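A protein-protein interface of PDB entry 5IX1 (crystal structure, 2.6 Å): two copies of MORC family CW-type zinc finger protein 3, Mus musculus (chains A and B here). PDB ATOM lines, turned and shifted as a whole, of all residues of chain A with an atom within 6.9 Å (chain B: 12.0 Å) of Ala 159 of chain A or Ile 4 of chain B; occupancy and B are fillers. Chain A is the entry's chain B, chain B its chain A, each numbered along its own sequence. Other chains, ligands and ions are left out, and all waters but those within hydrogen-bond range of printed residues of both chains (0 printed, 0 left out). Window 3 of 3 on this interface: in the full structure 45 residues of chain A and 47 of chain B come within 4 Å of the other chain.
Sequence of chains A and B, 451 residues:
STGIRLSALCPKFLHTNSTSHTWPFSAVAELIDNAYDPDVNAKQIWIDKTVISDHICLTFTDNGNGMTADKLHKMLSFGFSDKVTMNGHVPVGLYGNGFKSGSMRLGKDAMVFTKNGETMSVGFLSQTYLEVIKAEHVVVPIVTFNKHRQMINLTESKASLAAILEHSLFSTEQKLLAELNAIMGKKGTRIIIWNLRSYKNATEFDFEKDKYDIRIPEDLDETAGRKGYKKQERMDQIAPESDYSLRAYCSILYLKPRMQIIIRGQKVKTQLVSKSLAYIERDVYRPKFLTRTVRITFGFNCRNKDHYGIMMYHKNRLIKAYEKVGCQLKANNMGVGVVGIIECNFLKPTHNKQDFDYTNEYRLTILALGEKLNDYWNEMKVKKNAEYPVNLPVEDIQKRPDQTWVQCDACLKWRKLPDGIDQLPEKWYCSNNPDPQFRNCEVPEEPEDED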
ATOM      1  N   TYR A 129     -11.119   2.580  21.021  1.00  0.00           N
ATOM      2  CA  TYR A 129     -10.193   1.878  21.866  1.00  0.00           C
ATOM      3  C   TYR A 129      -9.356   2.865  22.621  1.00  0.00           C
ATOM      4  O   TYR A 129      -9.127   2.734  23.797  1.00  0.00           O
ATOM      5  CB  TYR A 129      -9.302   1.034  20.984  1.00  0.00           C
ATOM      6  CG  TYR A 129      -8.043   0.520  21.610  1.00  0.00           C
ATOM      7  CD1 TYR A 129      -8.057  -0.085  22.831  1.00  0.00           C
ATOM      8  CD2 TYR A 129      -6.850   0.612  20.954  1.00  0.00           C
ATOM      9  CE1 TYR A 129      -6.911  -0.574  23.389  1.00  0.00           C
ATOM     10  CE2 TYR A 129      -5.704   0.125  21.505  1.00  0.00           C
ATOM     11  CZ  TYR A 129      -5.744  -0.456  22.723  1.00  0.00           C
ATOM     12  OH  TYR A 129      -4.600  -0.937  23.265  1.00  0.00           O
ATOM     13  N   ILE A 133      -9.262   3.330  26.951  1.00  0.00           N
ATOM     14  CA  ILE A 133      -8.104   3.112  27.786  1.00  0.00           C
ATOM     15  C   ILE A 133      -7.410   4.417  28.088  1.00  0.00           C
ATOM     16  O   ILE A 133      -6.395   4.446  28.759  1.00  0.00           O
ATOM     17  CB  ILE A 133      -7.118   2.133  27.175  1.00  0.00           C
ATOM     18  CG1 ILE A 133      -6.636   2.632  25.836  1.00  0.00           C
ATOM     19  CG2 ILE A 133      -7.761   0.779  27.036  1.00  0.00           C
ATOM     20  CD1 ILE A 133      -5.340   2.002  25.421  1.00  0.00           C
ATOM     21  N   VAL A 139      -1.473   4.318  19.914  1.00  0.00           N
ATOM     22  CA  VAL A 139      -0.862   3.013  19.861  1.00  0.00           C
ATOM     23  C   VAL A 139      -1.646   2.137  18.916  1.00  0.00           C
ATOM     24  O   VAL A 139      -2.852   2.131  18.938  1.00  0.00           O
ATOM     25  CB  VAL A 139      -0.867   2.356  21.227  1.00  0.00           C
ATOM     26  CG1 VAL A 139       0.173   2.993  22.095  1.00  0.00           C
ATOM     27  CG2 VAL A 139      -2.223   2.500  21.863  1.00  0.00           C
ATOM     28  N   VAL A 140      -0.949   1.424  18.057  1.00  0.00           N
ATOM     29  CA  VAL A 140      -1.611   0.576  17.108  1.00  0.00           C
ATOM     30  C   VAL A 140      -1.302  -0.903  17.316  1.00  0.00           C
ATOM     31  O   VAL A 140      -0.287  -1.401  16.884  1.00  0.00           O
ATOM     32  CB  VAL A 140      -1.234   1.026  15.705  1.00  0.00           C
ATOM     33  CG1 VAL A 140      -1.946   2.315  15.391  1.00  0.00           C
ATOM     34  CG2 VAL A 140       0.252   1.258  15.614  1.00  0.00           C
ATOM     35  N   PRO A 141      -2.304  -1.621  17.985  1.00  0.00           N
ATOM     36  CA  PRO A 141      -1.966  -3.028  18.234  1.00  0.00           C
ATOM     37  C   PRO A 141      -1.776  -3.889  17.010  1.00  0.00           C
ATOM     38  O   PRO A 141      -2.518  -3.773  16.072  1.00  0.00           O
ATOM     39  CB  PRO A 141      -3.179  -3.543  18.967  1.00  0.00           C
ATOM     40  CG  PRO A 141      -3.647  -2.398  19.733  1.00  0.00           C
ATOM     41  CD  PRO A 141      -3.659  -1.380  18.683  1.00  0.00           C
ATOM     42  N   ILE A 142      -0.784  -4.759  17.030  1.00  0.00           N
ATOM     43  CA  ILE A 142      -0.548  -5.626  15.903  1.00  0.00           C
ATOM     44  C   ILE A 142      -0.277  -7.069  16.293  1.00  0.00           C
ATOM     45  O   ILE A 142       0.528  -7.333  17.156  1.00  0.00           O
ATOM     46  CB  ILE A 142       0.586  -5.082  15.053  1.00  0.00           C
ATOM     47  CG1 ILE A 142       0.160  -3.767  14.442  1.00  0.00           C
ATOM     48  CG2 ILE A 142       0.943  -6.034  13.936  1.00  0.00           C
ATOM     49  CD1 ILE A 142       1.155  -3.227  13.455  1.00  0.00           C
ATOM     50  N   VAL A 143      -0.929  -7.994  15.605  1.00  0.00           N
ATOM     51  CA  VAL A 143      -0.717  -9.411  15.820  1.00  0.00           C
ATOM     52  C   VAL A 143      -0.226 -10.044  14.549  1.00  0.00           C
ATOM     53  O   VAL A 143      -0.758  -9.785  13.501  1.00  0.00           O
ATOM     54  CB  VAL A 143      -2.003 -10.118  16.204  1.00  0.00           C
ATOM     55  CG1 VAL A 143      -1.682 -11.501  16.687  1.00  0.00           C
ATOM     56  CG2 VAL A 143      -2.712  -9.362  17.296  1.00  0.00           C
ATOM     57  N   MET A 151       1.458 -17.849  16.226  1.00  0.00           N
ATOM     58  CA  MET A 151       1.802 -16.505  16.659  1.00  0.00           C
ATOM     59  C   MET A 151       3.294 -16.283  16.685  1.00  0.00           C
ATOM     60  O   MET A 151       4.041 -17.194  16.927  1.00  0.00           O
ATOM     61  CB  MET A 151       1.246 -16.262  18.047  1.00  0.00           C
ATOM     62  CG  MET A 151       1.240 -14.816  18.463  1.00  0.00           C
ATOM     63  SD  MET A 151      -0.224 -14.401  19.397  1.00  0.00           S
ATOM     64  CE  MET A 151       0.456 -14.093  21.006  1.00  0.00           C
ATOM     65  N   LEU A 154       6.127 -12.376  19.696  1.00  0.00           N
ATOM     66  CA  LEU A 154       5.121 -12.680  20.685  1.00  0.00           C
ATOM     67  C   LEU A 154       4.790 -11.588  21.671  1.00  0.00           C
ATOM     68  O   LEU A 154       3.630 -11.407  22.004  1.00  0.00           O
ATOM     69  CB  LEU A 154       5.486 -13.956  21.435  1.00  0.00           C
ATOM     70  CG  LEU A 154       4.855 -15.228  20.868  1.00  0.00           C
ATOM     71  CD1 LEU A 154       5.890 -16.081  20.162  1.00  0.00           C
ATOM     72  CD2 LEU A 154       4.170 -16.034  21.954  1.00  0.00           C
ATOM     73  N   THR A 155       5.786 -10.866  22.148  1.00  0.00           N
ATOM     74  CA  THR A 155       5.527  -9.899  23.191  1.00  0.00           C
ATOM     75  C   THR A 155       4.579  -8.830  22.719  1.00  0.00           C
ATOM     76  O   THR A 155       3.648  -8.477  23.424  1.00  0.00           O
ATOM     77  CB  THR A 155       6.815  -9.229  23.622  1.00  0.00           C
ATOM     78  OG1 THR A 155       7.896  -9.791  22.879  1.00  0.00           O
ATOM     79  CG2 THR A 155       7.046  -9.463  25.086  1.00  0.00           C
ATOM     80  N   GLU A 156       4.810  -8.315  21.520  1.00  0.00           N
ATOM     81  CA  GLU A 156       3.898  -7.349  20.935  1.00  0.00           C
ATOM     82  C   GLU A 156       2.554  -7.947  20.630  1.00  0.00           C
ATOM     83  O   GLU A 156       1.525  -7.388  20.964  1.00  0.00           O
ATOM     84  CB  GLU A 156       4.481  -6.771  19.651  1.00  0.00           C
ATOM     85  CG  GLU A 156       3.511  -5.877  18.916  1.00  0.00           C
ATOM     86  CD  GLU A 156       4.023  -5.406  17.585  1.00  0.00           C
ATOM     87  OE1 GLU A 156       5.044  -5.922  17.121  1.00  0.00           O
ATOM     88  OE2 GLU A 156       3.399  -4.509  17.006  1.00  0.00           O
ATOM     89  N   SER A 157       2.577  -9.117  20.014  1.00  0.00           N
ATOM     90  CA  SER A 157       1.363  -9.775  19.586  1.00  0.00           C
ATOM     91  C   SER A 157       0.529 -10.147  20.765  1.00  0.00           C
ATOM     92  O   SER A 157      -0.680 -10.023  20.755  1.00  0.00           O
ATOM     93  CB  SER A 157       1.698 -11.009  18.783  1.00  0.00           C
ATOM     94  OG  SER A 157       2.604 -10.696  17.754  1.00  0.00           O
ATOM     95  N   LYS A 158       1.195 -10.615  21.796  1.00  0.00           N
ATOM     96  CA  LYS A 158       0.496 -11.076  22.947  1.00  0.00           C
ATOM     97  C   LYS A 158      -0.250  -9.915  23.530  1.00  0.00           C
ATOM     98  O   LYS A 158      -1.428 -10.011  23.790  1.00  0.00           O
ATOM     99  CB  LYS A 158       1.521 -11.614  23.931  1.00  0.00           C
ATOM    100  CG  LYS A 158       0.989 -12.106  25.263  1.00  0.00           C
ATOM    101  CD  LYS A 158       2.126 -12.696  26.088  1.00  0.00           C
ATOM    102  CE  LYS A 158       2.233 -12.067  27.470  1.00  0.00           C
ATOM    103  NZ  LYS A 158       3.584 -12.228  28.081  1.00  0.00           N
ATOM    104  N   ALA A 159       0.415  -8.789  23.683  1.00  0.00           N
ATOM    105  CA  ALA A 159      -0.266  -7.601  24.168  1.00  0.00           C
ATOM    106  C   ALA A 159      -1.272  -7.086  23.161  1.00  0.00           C
ATOM    107  O   ALA A 159      -2.373  -6.703  23.498  1.00  0.00           O
ATOM    108  CB  ALA A 159       0.731  -6.525  24.530  1.00  0.00           C
ATOM    109  N   SER A 160      -0.866  -7.106  21.907  1.00  0.00           N
ATOM    110  CA  SER A 160      -1.686  -6.531  20.886  1.00  0.00           C
ATOM    111  C   SER A 160      -2.961  -7.324  20.854  1.00  0.00           C
ATOM    112  O   SER A 160      -4.038  -6.771  20.829  1.00  0.00           O
ATOM    113  CB  SER A 160      -0.961  -6.639  19.549  1.00  0.00           C
ATOM    114  OG  SER A 160       0.165  -5.786  19.460  1.00  0.00           O
ATOM    115  N   LEU A 161      -2.839  -8.624  20.909  1.00  0.00           N
ATOM    116  CA  LEU A 161      -3.979  -9.515  20.779  1.00  0.00           C
ATOM    117  C   LEU A 161      -4.965  -9.363  21.885  1.00  0.00           C
ATOM    118  O   LEU A 161      -6.149  -9.396  21.676  1.00  0.00           O
ATOM    119  CB  LEU A 161      -3.518 -10.954  20.736  1.00  0.00           C
ATOM    120  CG  LEU A 161      -4.625 -12.001  20.820  1.00  0.00           C
ATOM    121  CD1 LEU A 161      -5.852 -11.548  20.066  1.00  0.00           C
ATOM    122  CD2 LEU A 161      -4.140 -13.322  20.271  1.00  0.00           C
ATOM    123  N   ALA A 162      -4.460  -9.196  23.083  1.00  0.00           N
ATOM    124  CA  ALA A 162      -5.312  -9.086  24.229  1.00  0.00           C
ATOM    125  C   ALA A 162      -6.179  -7.878  24.055  1.00  0.00           C
ATOM    126  O   ALA A 162      -7.347  -7.896  24.381  1.00  0.00           O
ATOM    127  CB  ALA A 162      -4.468  -8.937  25.460  1.00  0.00           C
ATOM    128  N   ALA A 163      -5.586  -6.811  23.550  1.00  0.00           N
ATOM    129  CA  ALA A 163      -6.310  -5.586  23.305  1.00  0.00           C
ATOM    130  C   ALA A 163      -7.384  -5.742  22.258  1.00  0.00           C
ATOM    131  O   ALA A 163      -8.491  -5.274  22.426  1.00  0.00           O
ATOM    132  CB  ALA A 163      -5.339  -4.508  22.881  1.00  0.00           C
ATOM    133  N   ILE A 164      -7.054  -6.419  21.177  1.00  0.00           N
ATOM    134  CA  ILE A 164      -7.988  -6.559  20.088  1.00  0.00           C
ATOM    135  C   ILE A 164      -9.223  -7.315  20.533  1.00  0.00           C
ATOM    136  O   ILE A 164     -10.329  -6.941  20.198  1.00  0.00           O
ATOM    137  CB  ILE A 164      -7.323  -7.295  18.924  1.00  0.00           C
ATOM    138  CG1 ILE A 164      -6.276  -6.407  18.301  1.00  0.00           C
ATOM    139  CG2 ILE A 164      -8.321  -7.702  17.860  1.00  0.00           C
ATOM    140  CD1 ILE A 164      -5.655  -7.000  17.073  1.00  0.00           C
ATOM    141  N   GLY B   3       3.559  -3.782  25.287  1.00  0.00           N
ATOM    142  CA  GLY B   3       4.395  -4.155  24.164  1.00  0.00           C
ATOM    143  C   GLY B   3       3.808  -3.682  22.858  1.00  0.00           C
ATOM    144  O   GLY B   3       4.372  -3.881  21.798  1.00  0.00           O
ATOM    145  N   ILE B   4       2.653  -3.054  22.951  1.00  0.00           N
ATOM    146  CA  ILE B   4       2.016  -2.466  21.807  1.00  0.00           C
ATOM    147  C   ILE B   4       2.763  -1.250  21.312  1.00  0.00           C
ATOM    148  O   ILE B   4       3.173  -0.412  22.083  1.00  0.00           O
ATOM    149  CB  ILE B   4       0.622  -2.019  22.177  1.00  0.00           C
ATOM    150  CG1 ILE B   4      -0.125  -3.160  22.829  1.00  0.00           C
ATOM    151  CG2 ILE B   4      -0.114  -1.571  20.946  1.00  0.00           C
ATOM    152  CD1 ILE B   4      -1.486  -2.761  23.327  1.00  0.00           C
ATOM    153  N   ARG B   5       2.922  -1.155  20.008  1.00  0.00           N
ATOM    154  CA  ARG B   5       3.647  -0.058  19.421  1.00  0.00           C
ATOM    155  C   ARG B   5       2.910   1.251  19.364  1.00  0.00           C
ATOM    156  O   ARG B   5       1.704   1.295  19.270  1.00  0.00           O
ATOM    157  CB  ARG B   5       4.115  -0.430  18.041  1.00  0.00           C
ATOM    158  CG  ARG B   5       5.548  -0.866  18.030  1.00  0.00           C
ATOM    159  CD  ARG B   5       5.761  -1.931  17.001  1.00  0.00           C
ATOM    160  NE  ARG B   5       6.505  -1.414  15.877  1.00  0.00           N
ATOM    161  CZ  ARG B   5       7.625  -0.734  15.993  1.00  0.00           C
ATOM    162  NH1 ARG B   5       8.251  -0.298  14.920  1.00  0.00           N
ATOM    163  NH2 ARG B   5       8.117  -0.511  17.186  1.00  0.00           N
ATOM    164  N   LEU B   6       3.670   2.328  19.430  1.00  0.00           N
ATOM    165  CA  LEU B   6       3.169   3.656  19.183  1.00  0.00           C
ATOM    166  C   LEU B   6       3.142   3.908  17.717  1.00  0.00           C
ATOM    167  O   LEU B   6       4.041   3.518  17.011  1.00  0.00           O
ATOM    168  CB  LEU B   6       4.105   4.684  19.771  1.00  0.00           C
ATOM    169  CG  LEU B   6       4.278   4.822  21.264  1.00  0.00           C
ATOM    170  CD1 LEU B   6       5.483   5.691  21.457  1.00  0.00           C
ATOM    171  CD2 LEU B   6       3.076   5.474  21.891  1.00  0.00           C
ATOM    172  N   SER B   7       2.128   4.614  17.264  1.00  0.00           N
ATOM    173  CA  SER B   7       2.115   5.079  15.904  1.00  0.00           C
ATOM    174  C   SER B   7       3.202   6.111  15.743  1.00  0.00           C
ATOM    175  O   SER B   7       3.466   6.868  16.641  1.00  0.00           O
ATOM    176  CB  SER B   7       0.775   5.681  15.563  1.00  0.00           C
ATOM    177  OG  SER B   7       0.749   6.025  14.210  1.00  0.00           O
ATOM    178  N   ALA B   8       3.810   6.145  14.577  1.00  0.00           N
ATOM    179  CA  ALA B   8       4.985   6.931  14.341  1.00  0.00           C
ATOM    180  C   ALA B   8       4.734   8.094  13.414  1.00  0.00           C
ATOM    181  O   ALA B   8       3.805   8.079  12.653  1.00  0.00           O
ATOM    182  CB  ALA B   8       6.063   6.059  13.771  1.00  0.00           C
ATOM    183  N   HIS B 137      12.082   9.879  12.396  1.00  0.00           N
ATOM    184  CA  HIS B 137      10.949  10.304  13.175  1.00  0.00           C
ATOM    185  C   HIS B 137      11.016  11.793  13.296  1.00  0.00           C
ATOM    186  O   HIS B 137      12.057  12.372  13.109  1.00  0.00           O
ATOM    187  CB  HIS B 137      10.991   9.703  14.562  1.00  0.00           C
ATOM    188  CG  HIS B 137      10.737   8.238  14.593  1.00  0.00           C
ATOM    189  ND1 HIS B 137      11.650   7.321  14.138  1.00  0.00           N
ATOM    190  CD2 HIS B 137       9.679   7.527  15.033  1.00  0.00           C
ATOM    191  CE1 HIS B 137      11.163   6.107  14.286  1.00  0.00           C
ATOM    192  NE2 HIS B 137       9.969   6.205  14.833  1.00  0.00           N
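The backbone NH of Val 140 of chain A sits at hydrogen-bond distance from the backbone carbonyl oxygen of Arg 5 of chain B (2.9 Å).
O of Glu 156 of chain A lies within hydrogen-bond range of OG of Ser 160 of chain A, at 2.6 Å.
Among the printed residues, merely in contact across the chains: Val 139 of chain A with Arg 5 of chain B (3.1 Å), Glu 156 of chain A with Arg 5 of chain B (3.5 Å), Pro 141 of chain A with Ile 4 of chain B (3.6 Å), Glu 156 of chain A with Gly 3 of chain B (3.6 Å), Tyr 129 of chain A with Ile 4 of chain B (3.6 Å), Val 139 of chain A with Leu 6 of chain B (3.8 Å), Ala 159 of chain A with Ile 4 of chain B (3.9 Å) and Val 140 of chain A with Ile 4 of chain B (3.9 Å).
Of the printed residues of chain B, Val 140 of chain A touches Ile 4 and Arg 5.
Of chain B, only Ile 4 (3.6 Å) comes within 4 Å of Pro 141 of chain A.
Of chain B, only Gly 3 and Arg 5 come within 4 Å of Glu 156 of chain A.
No residue of chain B comes within 4 Å of Ser 157 of chain A.
No residue of chain B comes within 4 Å of Ala 163 of chain A.
Of the printed residues of chain A, Ile 4 of chain B touches Tyr 129, Val 140, Pro 141 and Ala 159.
Of the printed residues of chain A, Arg 5 of chain B touches Val 139 (3.1 Å), Val 140 (2.9 Å) and Glu 156 (3.5 Å).
Of the printed residues of chain A, Leu 6 of chain B touches Val 139.
The nearest printed residue of chain B that does not touch Ala 159 of chain A is Gly 3 of chain B (4.01 Å).
Of the 19 printed residues of chain A, 6 touch a printed residue of chain B.
Printed residues of chain B that touch a printed residue of chain A: Gly 3, Ile 4, Arg 5 and Leu 6.
Hydrophobic or aromatic side chains of chain B that line the printed part of chain A: Ile 4 and Leu 6.
No position is printed for both chains.
Of the 9 pairs that touch across the chains among the printed residues, none has its exchanged pair printed and touching as well.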
